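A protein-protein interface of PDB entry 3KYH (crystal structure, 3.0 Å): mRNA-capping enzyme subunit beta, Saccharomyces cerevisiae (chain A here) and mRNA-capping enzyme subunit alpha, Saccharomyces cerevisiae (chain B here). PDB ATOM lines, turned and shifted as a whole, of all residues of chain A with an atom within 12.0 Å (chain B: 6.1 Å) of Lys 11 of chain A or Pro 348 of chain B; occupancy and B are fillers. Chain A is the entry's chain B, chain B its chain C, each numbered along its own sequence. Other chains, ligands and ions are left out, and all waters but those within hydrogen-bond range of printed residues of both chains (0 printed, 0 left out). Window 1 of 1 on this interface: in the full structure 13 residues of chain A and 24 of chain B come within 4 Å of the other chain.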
ATOM      1  N   PRO A   6       6.585 -32.491 -15.472  1.00  0.00           N
ATOM      2  CA  PRO A   6       5.707 -33.319 -16.284  1.00  0.00           C
ATOM      3  C   PRO A   6       4.704 -32.504 -17.109  1.00  0.00           C
ATOM      4  O   PRO A   6       5.029 -31.439 -17.656  1.00  0.00           O
ATOM      5  CB  PRO A   6       4.965 -34.164 -15.234  1.00  0.00           C
ATOM      6  CG  PRO A   6       4.950 -33.313 -14.023  1.00  0.00           C
ATOM      7  CD  PRO A   6       6.302 -32.647 -14.030  1.00  0.00           C
ATOM      8  N   ILE A   7       3.512 -33.086 -17.235  1.00  0.00           N
ATOM      9  CA  ILE A   7       2.314 -32.472 -17.809  1.00  0.00           C
ATOM     10  C   ILE A   7       2.087 -31.030 -17.384  1.00  0.00           C
ATOM     11  O   ILE A   7       1.978 -30.161 -18.243  1.00  0.00           O
ATOM     12  CB  ILE A   7       1.048 -33.347 -17.557  1.00  0.00           C
ATOM     13  CG1 ILE A   7       1.144 -34.147 -16.240  1.00  0.00           C
ATOM     14  CG2 ILE A   7       0.895 -34.355 -18.697  1.00  0.00           C
ATOM     15  CD1 ILE A   7       1.038 -33.354 -14.921  1.00  0.00           C
ATOM     16  N   TRP A   8       2.059 -30.778 -16.073  1.00  0.00           N
ATOM     17  CA  TRP A   8       1.842 -29.430 -15.564  1.00  0.00           C
ATOM     18  C   TRP A   8       2.761 -28.457 -16.295  1.00  0.00           C
ATOM     19  O   TRP A   8       2.272 -27.561 -16.987  1.00  0.00           O
ATOM     20  CB  TRP A   8       2.022 -29.335 -14.045  1.00  0.00           C
ATOM     21  CG  TRP A   8       1.021 -30.104 -13.190  1.00  0.00           C
ATOM     22  CD1 TRP A   8      -0.265 -30.501 -13.524  1.00  0.00           C
ATOM     23  CD2 TRP A   8       1.213 -30.477 -11.814  1.00  0.00           C
ATOM     24  NE1 TRP A   8      -0.846 -31.159 -12.459  1.00  0.00           N
ATOM     25  CE2 TRP A   8       0.032 -31.144 -11.394  1.00  0.00           C
ATOM     26  CE3 TRP A   8       2.284 -30.331 -10.901  1.00  0.00           C
ATOM     27  CZ2 TRP A   8      -0.101 -31.676 -10.103  1.00  0.00           C
ATOM     28  CZ3 TRP A   8       2.152 -30.863  -9.620  1.00  0.00           C
ATOM     29  CH2 TRP A   8       0.966 -31.521  -9.231  1.00  0.00           C
ATOM     30  N   ALA A   9       4.070 -28.701 -16.214  1.00  0.00           N
ATOM     31  CA  ALA A   9       5.085 -27.909 -16.915  1.00  0.00           C
ATOM     32  C   ALA A   9       4.730 -27.636 -18.374  1.00  0.00           C
ATOM     33  O   ALA A   9       4.838 -26.493 -18.815  1.00  0.00           O
ATOM     34  CB  ALA A   9       6.456 -28.568 -16.808  1.00  0.00           C
ATOM     35  N   GLN A  10       4.254 -28.673 -19.075  1.00  0.00           N
ATOM     36  CA  GLN A  10       3.836 -28.604 -20.491  1.00  0.00           C
ATOM     37  C   GLN A  10       2.721 -27.575 -20.737  1.00  0.00           C
ATOM     38  O   GLN A  10       1.789 -27.418 -19.933  1.00  0.00           O
ATOM     39  CB  GLN A  10       3.397 -29.981 -21.021  1.00  0.00           C
ATOM     40  CG  GLN A  10       4.464 -31.081 -20.988  1.00  0.00           C
ATOM     41  CD  GLN A  10       5.529 -30.915 -22.063  1.00  0.00           C
ATOM     42  OE1 GLN A  10       5.250 -30.994 -23.266  1.00  0.00           O
ATOM     43  NE2 GLN A  10       6.763 -30.685 -21.629  1.00  0.00           N
ATOM     44  N   LYS A  11       2.841 -26.870 -21.860  1.00  0.00           N
ATOM     45  CA  LYS A  11       1.928 -25.784 -22.214  1.00  0.00           C
ATOM     46  C   LYS A  11       0.580 -26.294 -22.727  1.00  0.00           C
ATOM     47  O   LYS A  11       0.532 -27.268 -23.490  1.00  0.00           O
ATOM     48  CB  LYS A  11       2.614 -24.845 -23.205  1.00  0.00           C
ATOM     49  CG  LYS A  11       3.848 -24.170 -22.597  1.00  0.00           C
ATOM     50  CD  LYS A  11       4.892 -23.746 -23.621  1.00  0.00           C
ATOM     51  CE  LYS A  11       4.454 -22.587 -24.512  1.00  0.00           C
ATOM     52  NZ  LYS A  11       4.364 -21.281 -23.784  1.00  0.00           N
ATOM     53  N   TRP A  12      -0.499 -25.651 -22.263  1.00  0.00           N
ATOM     54  CA  TRP A  12      -1.887 -26.016 -22.599  1.00  0.00           C
ATOM     55  C   TRP A  12      -2.105 -25.845 -24.085  1.00  0.00           C
ATOM     56  O   TRP A  12      -2.333 -24.741 -24.586  1.00  0.00           O
ATOM     57  CB  TRP A  12      -2.923 -25.250 -21.755  1.00  0.00           C
ATOM     58  CG  TRP A  12      -4.388 -25.432 -22.138  1.00  0.00           C
ATOM     59  CD1 TRP A  12      -5.011 -24.931 -23.246  1.00  0.00           C
ATOM     60  CD2 TRP A  12      -5.418 -26.074 -21.366  1.00  0.00           C
ATOM     61  NE1 TRP A  12      -6.342 -25.257 -23.241  1.00  0.00           N
ATOM     62  CE2 TRP A  12      -6.626 -25.949 -22.093  1.00  0.00           C
ATOM     63  CE3 TRP A  12      -5.436 -26.764 -20.145  1.00  0.00           C
ATOM     64  CZ2 TRP A  12      -7.837 -26.493 -21.647  1.00  0.00           C
ATOM     65  CZ3 TRP A  12      -6.643 -27.271 -19.685  1.00  0.00           C
ATOM     66  CH2 TRP A  12      -7.827 -27.145 -20.441  1.00  0.00           C
ATOM     67  N   LYS A  13      -1.897 -26.971 -24.760  1.00  0.00           N
ATOM     68  CA  LYS A  13      -2.146 -27.181 -26.180  1.00  0.00           C
ATOM     69  C   LYS A  13      -3.626 -27.309 -26.567  1.00  0.00           C
ATOM     70  O   LYS A  13      -3.943 -27.011 -27.726  1.00  0.00           O
ATOM     71  CB  LYS A  13      -1.380 -28.421 -26.665  1.00  0.00           C
ATOM     72  CG  LYS A  13      -0.051 -28.152 -27.355  1.00  0.00           C
ATOM     73  CD  LYS A  13       1.118 -27.854 -26.420  1.00  0.00           C
ATOM     74  CE  LYS A  13       1.520 -26.391 -26.485  1.00  0.00           C
ATOM     75  NZ  LYS A  13       2.276 -26.098 -27.733  1.00  0.00           N
ATOM     76  N   PRO A  14      -4.511 -27.789 -25.645  1.00  0.00           N
ATOM     77  CA  PRO A  14      -5.958 -27.833 -25.937  1.00  0.00           C
ATOM     78  C   PRO A  14      -6.591 -26.502 -26.380  1.00  0.00           C
ATOM     79  O   PRO A  14      -7.821 -26.373 -26.432  1.00  0.00           O
ATOM     80  CB  PRO A  14      -6.583 -28.357 -24.633  1.00  0.00           C
ATOM     81  CG  PRO A  14      -5.451 -28.695 -23.715  1.00  0.00           C
ATOM     82  CD  PRO A  14      -4.193 -28.681 -24.509  1.00  0.00           C
ATOM     83  N   THR A  15      -5.727 -25.537 -26.690  1.00  0.00           N
ATOM     84  CA  THR A  15      -6.026 -24.300 -27.399  1.00  0.00           C
ATOM     85  C   THR A  15      -6.518 -24.600 -28.822  1.00  0.00           C
ATOM     86  O   THR A  15      -5.867 -24.239 -29.806  1.00  0.00           O
ATOM     87  CB  THR A  15      -4.740 -23.435 -27.473  1.00  0.00           C
ATOM     88  OG1 THR A  15      -4.089 -23.412 -26.193  1.00  0.00           O
ATOM     89  CG2 THR A  15      -5.058 -22.011 -27.900  1.00  0.00           C
ATOM     90  N   ILE A  16      -7.670 -25.265 -28.913  1.00  0.00           N
ATOM     91  CA  ILE A  16      -8.317 -25.628 -30.183  1.00  0.00           C
ATOM     92  C   ILE A  16      -9.850 -25.606 -30.146  1.00  0.00           C
ATOM     93  O   ILE A  16     -10.480 -25.492 -31.200  1.00  0.00           O
ATOM     94  CB  ILE A  16      -7.810 -26.976 -30.803  1.00  0.00           C
ATOM     95  CG1 ILE A  16      -7.755 -28.126 -29.781  1.00  0.00           C
ATOM     96  CG2 ILE A  16      -6.475 -26.782 -31.525  1.00  0.00           C
ATOM     97  CD1 ILE A  16      -7.577 -29.521 -30.406  1.00  0.00           C
ATOM     98  N   LYS A  17     -10.439 -25.706 -28.949  1.00  0.00           N
ATOM     99  CA  LYS A  17     -11.903 -25.733 -28.787  1.00  0.00           C
ATOM    100  C   LYS A  17     -12.625 -24.377 -28.755  1.00  0.00           C
ATOM    101  O   LYS A  17     -13.823 -24.305 -29.043  1.00  0.00           O
ATOM    102  CB  LYS A  17     -12.349 -26.664 -27.642  1.00  0.00           C
ATOM    103  CG  LYS A  17     -11.982 -26.255 -26.212  1.00  0.00           C
ATOM    104  CD  LYS A  17     -12.623 -27.182 -25.154  1.00  0.00           C
ATOM    105  CE  LYS A  17     -14.116 -26.861 -24.912  1.00  0.00           C
ATOM    106  NZ  LYS A  17     -14.827 -27.747 -23.912  1.00  0.00           N
ATOM    107  N   ARG B 306       0.606 -19.137 -30.405  1.00  0.00           N
ATOM    108  CA  ARG B 306       0.301 -20.562 -30.606  1.00  0.00           C
ATOM    109  C   ARG B 306       1.049 -21.207 -31.770  1.00  0.00           C
ATOM    110  O   ARG B 306       1.408 -22.382 -31.696  1.00  0.00           O
ATOM    111  CB  ARG B 306      -1.208 -20.803 -30.754  1.00  0.00           C
ATOM    112  CG  ARG B 306      -2.140 -19.951 -29.871  1.00  0.00           C
ATOM    113  CD  ARG B 306      -1.909 -20.118 -28.379  1.00  0.00           C
ATOM    114  NE  ARG B 306      -1.608 -21.511 -28.070  1.00  0.00           N
ATOM    115  CZ  ARG B 306      -1.305 -21.985 -26.866  1.00  0.00           C
ATOM    116  NH1 ARG B 306      -1.256 -21.180 -25.808  1.00  0.00           N
ATOM    117  NH2 ARG B 306      -1.041 -23.281 -26.735  1.00  0.00           N
ATOM    118  N   HIS B 309       4.265 -21.813 -30.343  1.00  0.00           N
ATOM    119  CA  HIS B 309       4.046 -22.503 -29.070  1.00  0.00           C
ATOM    120  C   HIS B 309       4.278 -23.997 -29.198  1.00  0.00           C
ATOM    121  O   HIS B 309       4.773 -24.615 -28.256  1.00  0.00           O
ATOM    122  CB  HIS B 309       2.637 -22.269 -28.514  1.00  0.00           C
ATOM    123  CG  HIS B 309       2.496 -21.033 -27.678  1.00  0.00           C
ATOM    124  ND1 HIS B 309       3.550 -20.451 -27.008  1.00  0.00           N
ATOM    125  CD2 HIS B 309       1.398 -20.315 -27.340  1.00  0.00           C
ATOM    126  CE1 HIS B 309       3.116 -19.400 -26.333  1.00  0.00           C
ATOM    127  NE2 HIS B 309       1.810 -19.305 -26.506  1.00  0.00           N
ATOM    128  N   GLN B 312       7.837 -25.855 -28.630  1.00  0.00           N
ATOM    129  CA  GLN B 312       8.196 -25.804 -27.210  1.00  0.00           C
ATOM    130  C   GLN B 312       8.874 -27.074 -26.639  1.00  0.00           C
ATOM    131  O   GLN B 312       8.757 -28.166 -27.217  1.00  0.00           O
ATOM    132  CB  GLN B 312       6.951 -25.445 -26.367  1.00  0.00           C
ATOM    133  CG  GLN B 312       6.361 -26.540 -25.435  1.00  0.00           C
ATOM    134  CD  GLN B 312       5.528 -27.618 -26.123  1.00  0.00           C
ATOM    135  OE1 GLN B 312       4.686 -27.317 -26.973  1.00  0.00           O
ATOM    136  NE2 GLN B 312       5.719 -28.878 -25.707  1.00  0.00           N
ATOM    137  N   PRO B 313       9.673 -26.894 -25.560  1.00  0.00           N
ATOM    138  CA  PRO B 313       9.796 -27.914 -24.505  1.00  0.00           C
ATOM    139  C   PRO B 313       8.991 -27.508 -23.247  1.00  0.00           C
ATOM    140  O   PRO B 313       8.258 -28.331 -22.686  1.00  0.00           O
ATOM    141  CB  PRO B 313      11.305 -27.974 -24.226  1.00  0.00           C
ATOM    142  CG  PRO B 313      11.855 -26.661 -24.689  1.00  0.00           C
ATOM    143  CD  PRO B 313      10.844 -25.991 -25.591  1.00  0.00           C
ATOM    144  N   PHE B 314       9.105 -26.231 -22.866  1.00  0.00           N
ATOM    145  CA  PHE B 314       8.462 -25.585 -21.716  1.00  0.00           C
ATOM    146  C   PHE B 314       8.815 -24.090 -21.791  1.00  0.00           C
ATOM    147  O   PHE B 314       9.862 -23.727 -22.344  1.00  0.00           O
ATOM    148  CB  PHE B 314       8.940 -26.209 -20.398  1.00  0.00           C
ATOM    149  CG  PHE B 314       8.628 -25.387 -19.175  1.00  0.00           C
ATOM    150  CD1 PHE B 314       7.325 -25.303 -18.685  1.00  0.00           C
ATOM    151  CD2 PHE B 314       9.645 -24.704 -18.503  1.00  0.00           C
ATOM    152  CE1 PHE B 314       7.029 -24.547 -17.547  1.00  0.00           C
ATOM    153  CE2 PHE B 314       9.362 -23.937 -17.360  1.00  0.00           C
ATOM    154  CZ  PHE B 314       8.046 -23.860 -16.883  1.00  0.00           C
ATOM    155  N   ASP B 315       7.968 -23.248 -21.196  1.00  0.00           N
ATOM    156  CA  ASP B 315       7.982 -21.781 -21.364  1.00  0.00           C
ATOM    157  C   ASP B 315       9.275 -20.987 -21.110  1.00  0.00           C
ATOM    158  O   ASP B 315       9.403 -19.897 -21.658  1.00  0.00           O
ATOM    159  CB  ASP B 315       6.817 -21.145 -20.589  1.00  0.00           C
ATOM    160  CG  ASP B 315       6.185 -19.941 -21.317  1.00  0.00           C
ATOM    161  OD1 ASP B 315       6.892 -19.008 -21.759  1.00  0.00           O
ATOM    162  OD2 ASP B 315       4.941 -19.894 -21.421  1.00  0.00           O
ATOM    163  N   GLU B 318      10.224 -19.063 -24.143  1.00  0.00           N
ATOM    164  CA  GLU B 318       8.995 -18.558 -24.766  1.00  0.00           C
ATOM    165  C   GLU B 318       8.443 -17.250 -24.172  1.00  0.00           C
ATOM    166  O   GLU B 318       7.750 -16.495 -24.872  1.00  0.00           O
ATOM    167  CB  GLU B 318       7.931 -19.667 -24.751  1.00  0.00           C
ATOM    168  CG  GLU B 318       6.789 -19.518 -25.769  1.00  0.00           C
ATOM    169  CD  GLU B 318       7.118 -20.031 -27.180  1.00  0.00           C
ATOM    170  OE1 GLU B 318       8.296 -20.328 -27.489  1.00  0.00           O
ATOM    171  OE2 GLU B 318       6.172 -20.139 -27.996  1.00  0.00           O
ATOM    172  N   LEU B 322       6.080 -14.004 -26.152  1.00  0.00           N
ATOM    173  CA  LEU B 322       4.868 -13.988 -25.300  1.00  0.00           C
ATOM    174  C   LEU B 322       4.563 -12.677 -24.585  1.00  0.00           C
ATOM    175  O   LEU B 322       3.397 -12.321 -24.375  1.00  0.00           O
ATOM    176  CB  LEU B 322       4.962 -15.112 -24.258  1.00  0.00           C
ATOM    177  CG  LEU B 322       3.949 -15.365 -23.130  1.00  0.00           C
ATOM    178  CD1 LEU B 322       4.068 -16.828 -22.709  1.00  0.00           C
ATOM    179  CD2 LEU B 322       4.168 -14.440 -21.926  1.00  0.00           C
ATOM    180  N   GLU B 346      -5.265 -34.309 -14.192  1.00  0.00           N
ATOM    181  CA  GLU B 346      -4.453 -33.181 -14.654  1.00  0.00           C
ATOM    182  C   GLU B 346      -4.439 -33.120 -16.175  1.00  0.00           C
ATOM    183  O   GLU B 346      -5.024 -34.001 -16.819  1.00  0.00           O
ATOM    184  CB  GLU B 346      -3.024 -33.348 -14.123  1.00  0.00           C
ATOM    185  CG  GLU B 346      -1.996 -34.091 -15.012  1.00  0.00           C
ATOM    186  CD  GLU B 346      -2.322 -35.530 -15.448  1.00  0.00           C
ATOM    187  OE1 GLU B 346      -1.379 -36.194 -15.928  1.00  0.00           O
ATOM    188  OE2 GLU B 346      -3.464 -36.028 -15.325  1.00  0.00           O
ATOM    189  N   GLN B 347      -3.742 -32.109 -16.717  1.00  0.00           N
ATOM    190  CA  GLN B 347      -3.530 -31.835 -18.158  1.00  0.00           C
ATOM    191  C   GLN B 347      -2.592 -30.626 -18.288  1.00  0.00           C
ATOM    192  O   GLN B 347      -2.414 -29.923 -17.294  1.00  0.00           O
ATOM    193  CB  GLN B 347      -4.850 -31.604 -18.906  1.00  0.00           C
ATOM    194  CG  GLN B 347      -5.797 -30.567 -18.294  1.00  0.00           C
ATOM    195  CD  GLN B 347      -6.976 -30.233 -19.196  1.00  0.00           C
ATOM    196  OE1 GLN B 347      -6.863 -30.229 -20.426  1.00  0.00           O
ATOM    197  NE2 GLN B 347      -8.106 -29.913 -18.583  1.00  0.00           N
ATOM    198  N   PRO B 348      -1.997 -30.370 -19.484  1.00  0.00           N
ATOM    199  CA  PRO B 348      -0.919 -29.374 -19.541  1.00  0.00           C
ATOM    200  C   PRO B 348      -1.395 -27.994 -19.136  1.00  0.00           C
ATOM    201  O   PRO B 348      -2.504 -27.605 -19.520  1.00  0.00           O
ATOM    202  CB  PRO B 348      -0.472 -29.398 -21.010  1.00  0.00           C
ATOM    203  CG  PRO B 348      -1.620 -29.930 -21.753  1.00  0.00           C
ATOM    204  CD  PRO B 348      -2.238 -30.944 -20.827  1.00  0.00           C
ATOM    205  N   LEU B 349      -0.559 -27.279 -18.369  1.00  0.00           N
ATOM    206  CA  LEU B 349      -0.998 -26.070 -17.642  1.00  0.00           C
ATOM    207  C   LEU B 349      -0.469 -24.662 -17.905  1.00  0.00           C
ATOM    208  O   LEU B 349      -1.244 -23.688 -17.823  1.00  0.00           O
ATOM    209  CB  LEU B 349      -1.054 -26.359 -16.165  1.00  0.00           C
ATOM    210  CG  LEU B 349      -2.491 -26.818 -15.925  1.00  0.00           C
ATOM    211  CD1 LEU B 349      -2.573 -27.920 -14.849  1.00  0.00           C
ATOM    212  CD2 LEU B 349      -3.229 -25.586 -15.538  1.00  0.00           C
ATOM    213  N   ASN B 350       0.807 -24.590 -18.303  1.00  0.00           N
ATOM    214  CA  ASN B 350       1.564 -23.346 -18.482  1.00  0.00           C
ATOM    215  C   ASN B 350       0.980 -22.569 -19.639  1.00  0.00           C
ATOM    216  O   ASN B 350       1.630 -22.431 -20.683  1.00  0.00           O
ATOM    217  CB  ASN B 350       3.064 -23.647 -18.684  1.00  0.00           C
ATOM    218  CG  ASN B 350       3.954 -22.381 -18.678  1.00  0.00           C
ATOM    219  OD1 ASN B 350       3.915 -21.558 -19.597  1.00  0.00           O
ATOM    220  ND2 ASN B 350       4.795 -22.257 -17.649  1.00  0.00           N
ATOM    221  N   GLY B 351      -0.235 -22.053 -19.425  1.00  0.00           N
ATOM    222  CA  GLY B 351      -1.106 -21.595 -20.525  1.00  0.00           C
ATOM    223  C   GLY B 351      -2.584 -21.998 -20.567  1.00  0.00           C
ATOM    224  O   GLY B 351      -3.224 -21.854 -21.611  1.00  0.00           O
ATOM    225  N   ARG B 352      -3.132 -22.529 -19.475  1.00  0.00           N
ATOM    226  CA  ARG B 352      -4.596 -22.698 -19.352  1.00  0.00           C
ATOM    227  C   ARG B 352      -5.257 -21.428 -18.788  1.00  0.00           C
ATOM    228  O   ARG B 352      -4.552 -20.433 -18.554  1.00  0.00           O
ATOM    229  CB  ARG B 352      -4.937 -23.933 -18.505  1.00  0.00           C
ATOM    230  CG  ARG B 352      -5.545 -23.678 -17.152  1.00  0.00           C
ATOM    231  CD  ARG B 352      -7.066 -23.865 -17.131  1.00  0.00           C
ATOM    232  NE  ARG B 352      -7.567 -25.232 -17.244  1.00  0.00           N
ATOM    233  CZ  ARG B 352      -7.477 -26.154 -16.288  1.00  0.00           C
ATOM    234  NH1 ARG B 352      -6.853 -25.848 -15.170  1.00  0.00           N
ATOM    235  NH2 ARG B 352      -7.962 -27.392 -16.459  1.00  0.00           N
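NZ of Lys 13 of chain A is in hydrogen-bond range of O of His 309 of chain B (3.0 Å). The backbone NH (N) of Leu 349 of chain B sits at hydrogen-bond distance from the backbone carbonyl oxygen (O) of Trp 8 of chain A. The side-chain amino group (NZ) of Lys 13 of chain A sits at hydrogen-bond distance from the side-chain amide oxygen (OE1) of Gln 312 of chain B (2.8 Å). NZ of Lys 11 of chain A sits close to ND1 of His 309 of chain B, 3.4 Å away. NE2 of Gln 10 of chain A sits at hydrogen-bond distance from O of Pro 313 of chain B, at 3.0 Å. OE1 of Gln 10 of chain A is in hydrogen-bond range of NE2 of Gln 312 of chain B, 3.3 Å away. O of Gln 10 of chain A is in hydrogen-bond range of N of Leu 349 of chain B (2.8 Å). The backbone NH (N) of Asn 350 of chain B is in hydrogen-bond range of the backbone carbonyl oxygen (O) of Gln 10 of chain A, at 3.4 Å. The side-chain hydroxyl (OG1) of Thr 15 of chain A is in hydrogen-bond range of the guanidinium group (NH2) of Arg 306 of chain B (3.1 Å). The side-chain carboxylate (OD2) of Asp 315 of chain B is in salt-bridge range of the side-chain amino group (NZ) of Lys 11 of chain A, 2.8 Å away. The guanidinium group of Arg 306 of chain B is in hydrogen-bond range of the backbone carbonyl oxygen of Trp 12 of chain A, at 2.9 Å.
The side-chain carboxylate (OD2) of Asp 315 of chain B sits close to the side-chain amide oxygen (OD1) of Asn 350 of chain B, at 2.7 Å. The backbone carbonyl oxygen (O) of His 309 of chain B lies close to the side-chain amide oxygen (OE1) of Gln 312 of chain B, at 3.0 Å. A ring nitrogen (ND1) of His 309 of chain B is in hydrogen-bond range of the side-chain carboxylate (OE2) of Glu 318 of chain B (2.8 Å). The side-chain amide nitrogen (NE2) of Gln 347 of chain B sits close to the guanidinium group (NH2) of Arg 352 of chain B (3.3 Å). O of Trp 12 of chain A lies within hydrogen-bond range of OG1 of Thr 15 of chain A, at 2.7 Å.
Among the printed residues, pairs that only touch across the chains: Ile 7 of chain A with Glu 346 of chain B (3.1 Å), Ile 7 of chain A with Pro 348 of chain B (3.3 Å), Ile 7 of chain A with Leu 349 of chain B (3.8 Å), Trp 8 of chain A with Glu 346 of chain B (3.5 Å), Trp 8 of chain A with Asn 350 of chain B (3.6 Å), Ala 9 of chain A with Phe 314 of chain B (2.8 Å), Ala 9 of chain A with Asn 350 of chain B (3.4 Å), Gln 10 of chain A with Pro 348 of chain B (3.2 Å), Lys 11 of chain A with Gln 312 of chain B (3.6 Å), Lys 11 of chain A with Glu 318 of chain B (3.6 Å), Lys 11 of chain A with Pro 348 of chain B (3.4 Å), Lys 11 of chain A with Asn 350 of chain B (3.4 Å), Trp 12 of chain A with Gln 347 of chain B (3.0 Å), Trp 12 of chain A with Pro 348 of chain B (3.1 Å), Trp 12 of chain A with Gly 351 of chain B (3.4 Å), Trp 12 of chain A with Arg 352 of chain B (3.3 Å), Pro 14 of chain A with Gln 347 of chain B (3.9 Å) and Pro 14 of chain A with Pro 348 of chain B (3.97 Å).
Of the printed residues of chain B, Trp 8 of chain A touches Glu 346 (3.5 Å), Leu 349 (3.2 Å) and Asn 350 (3.6 Å). Of the printed residues of chain B, Ala 9 of chain A touches Phe 314 (2.8 Å) and Asn 350 (3.4 Å). Of chain B, only His 309, Gln 312, Asp 315, Glu 318, Pro 348 and Asn 350 come within 4 Å of Lys 11 of chain A. Printed residues of chain B within 4 Å of Pro 14 of chain A: Gln 347 and Pro 348. Of the printed residues of chain B, Thr 15 of chain A touches Arg 306. Lys 17 of chain A touches none of the printed residues of chain B. Printed residues of chain A within 4 Å of Arg 306 of chain B: Trp 12 (2.9 Å) and Thr 15 (3.1 Å). Gln 312 of chain B touches three residues of chain A. Of chain A, only Gln 10 (3.0 Å) comes within 4 Å of Pro 313 of chain B. Phe 314 of chain B touches just one residue of chain A: Ala 9. Of chain A, only Lys 11 comes within 4 Å of Asp 315 of chain B. Leu 322 of chain B touches none of the printed residues of chain A. Of chain A, only Trp 12 and Pro 14 come within 4 Å of Gln 347 of chain B. Pro 348 of chain B touches five residues of chain A. Of chain A, only Ile 7 (3.8 Å), Trp 8 (3.2 Å) and Gln 10 (2.8 Å) come within 4 Å of Leu 349 of chain B. Of chain A, only Trp 12 comes within 4 Å of Gly 351 of chain B. Arg 352 of chain B touches one residue of chain A. The nearest residue of chain B that does not touch Lys 11 of chain A is Phe 314 of chain B (4.3 Å). The nearest residue of chain A that does not touch Pro 348 of chain B is Lys 13 of chain A (4.2 Å).
Hydrophobic or aromatic side chains of chain B that line the printed part of chain A: His 309, Phe 314, Pro 348 and Leu 349. Among the printed residues, Asp or Glu carboxylates within 4 Å of a Lys or Arg side-chain nitrogen of the other chain: Lys 11 of chain A with Asp 315 of chain B.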
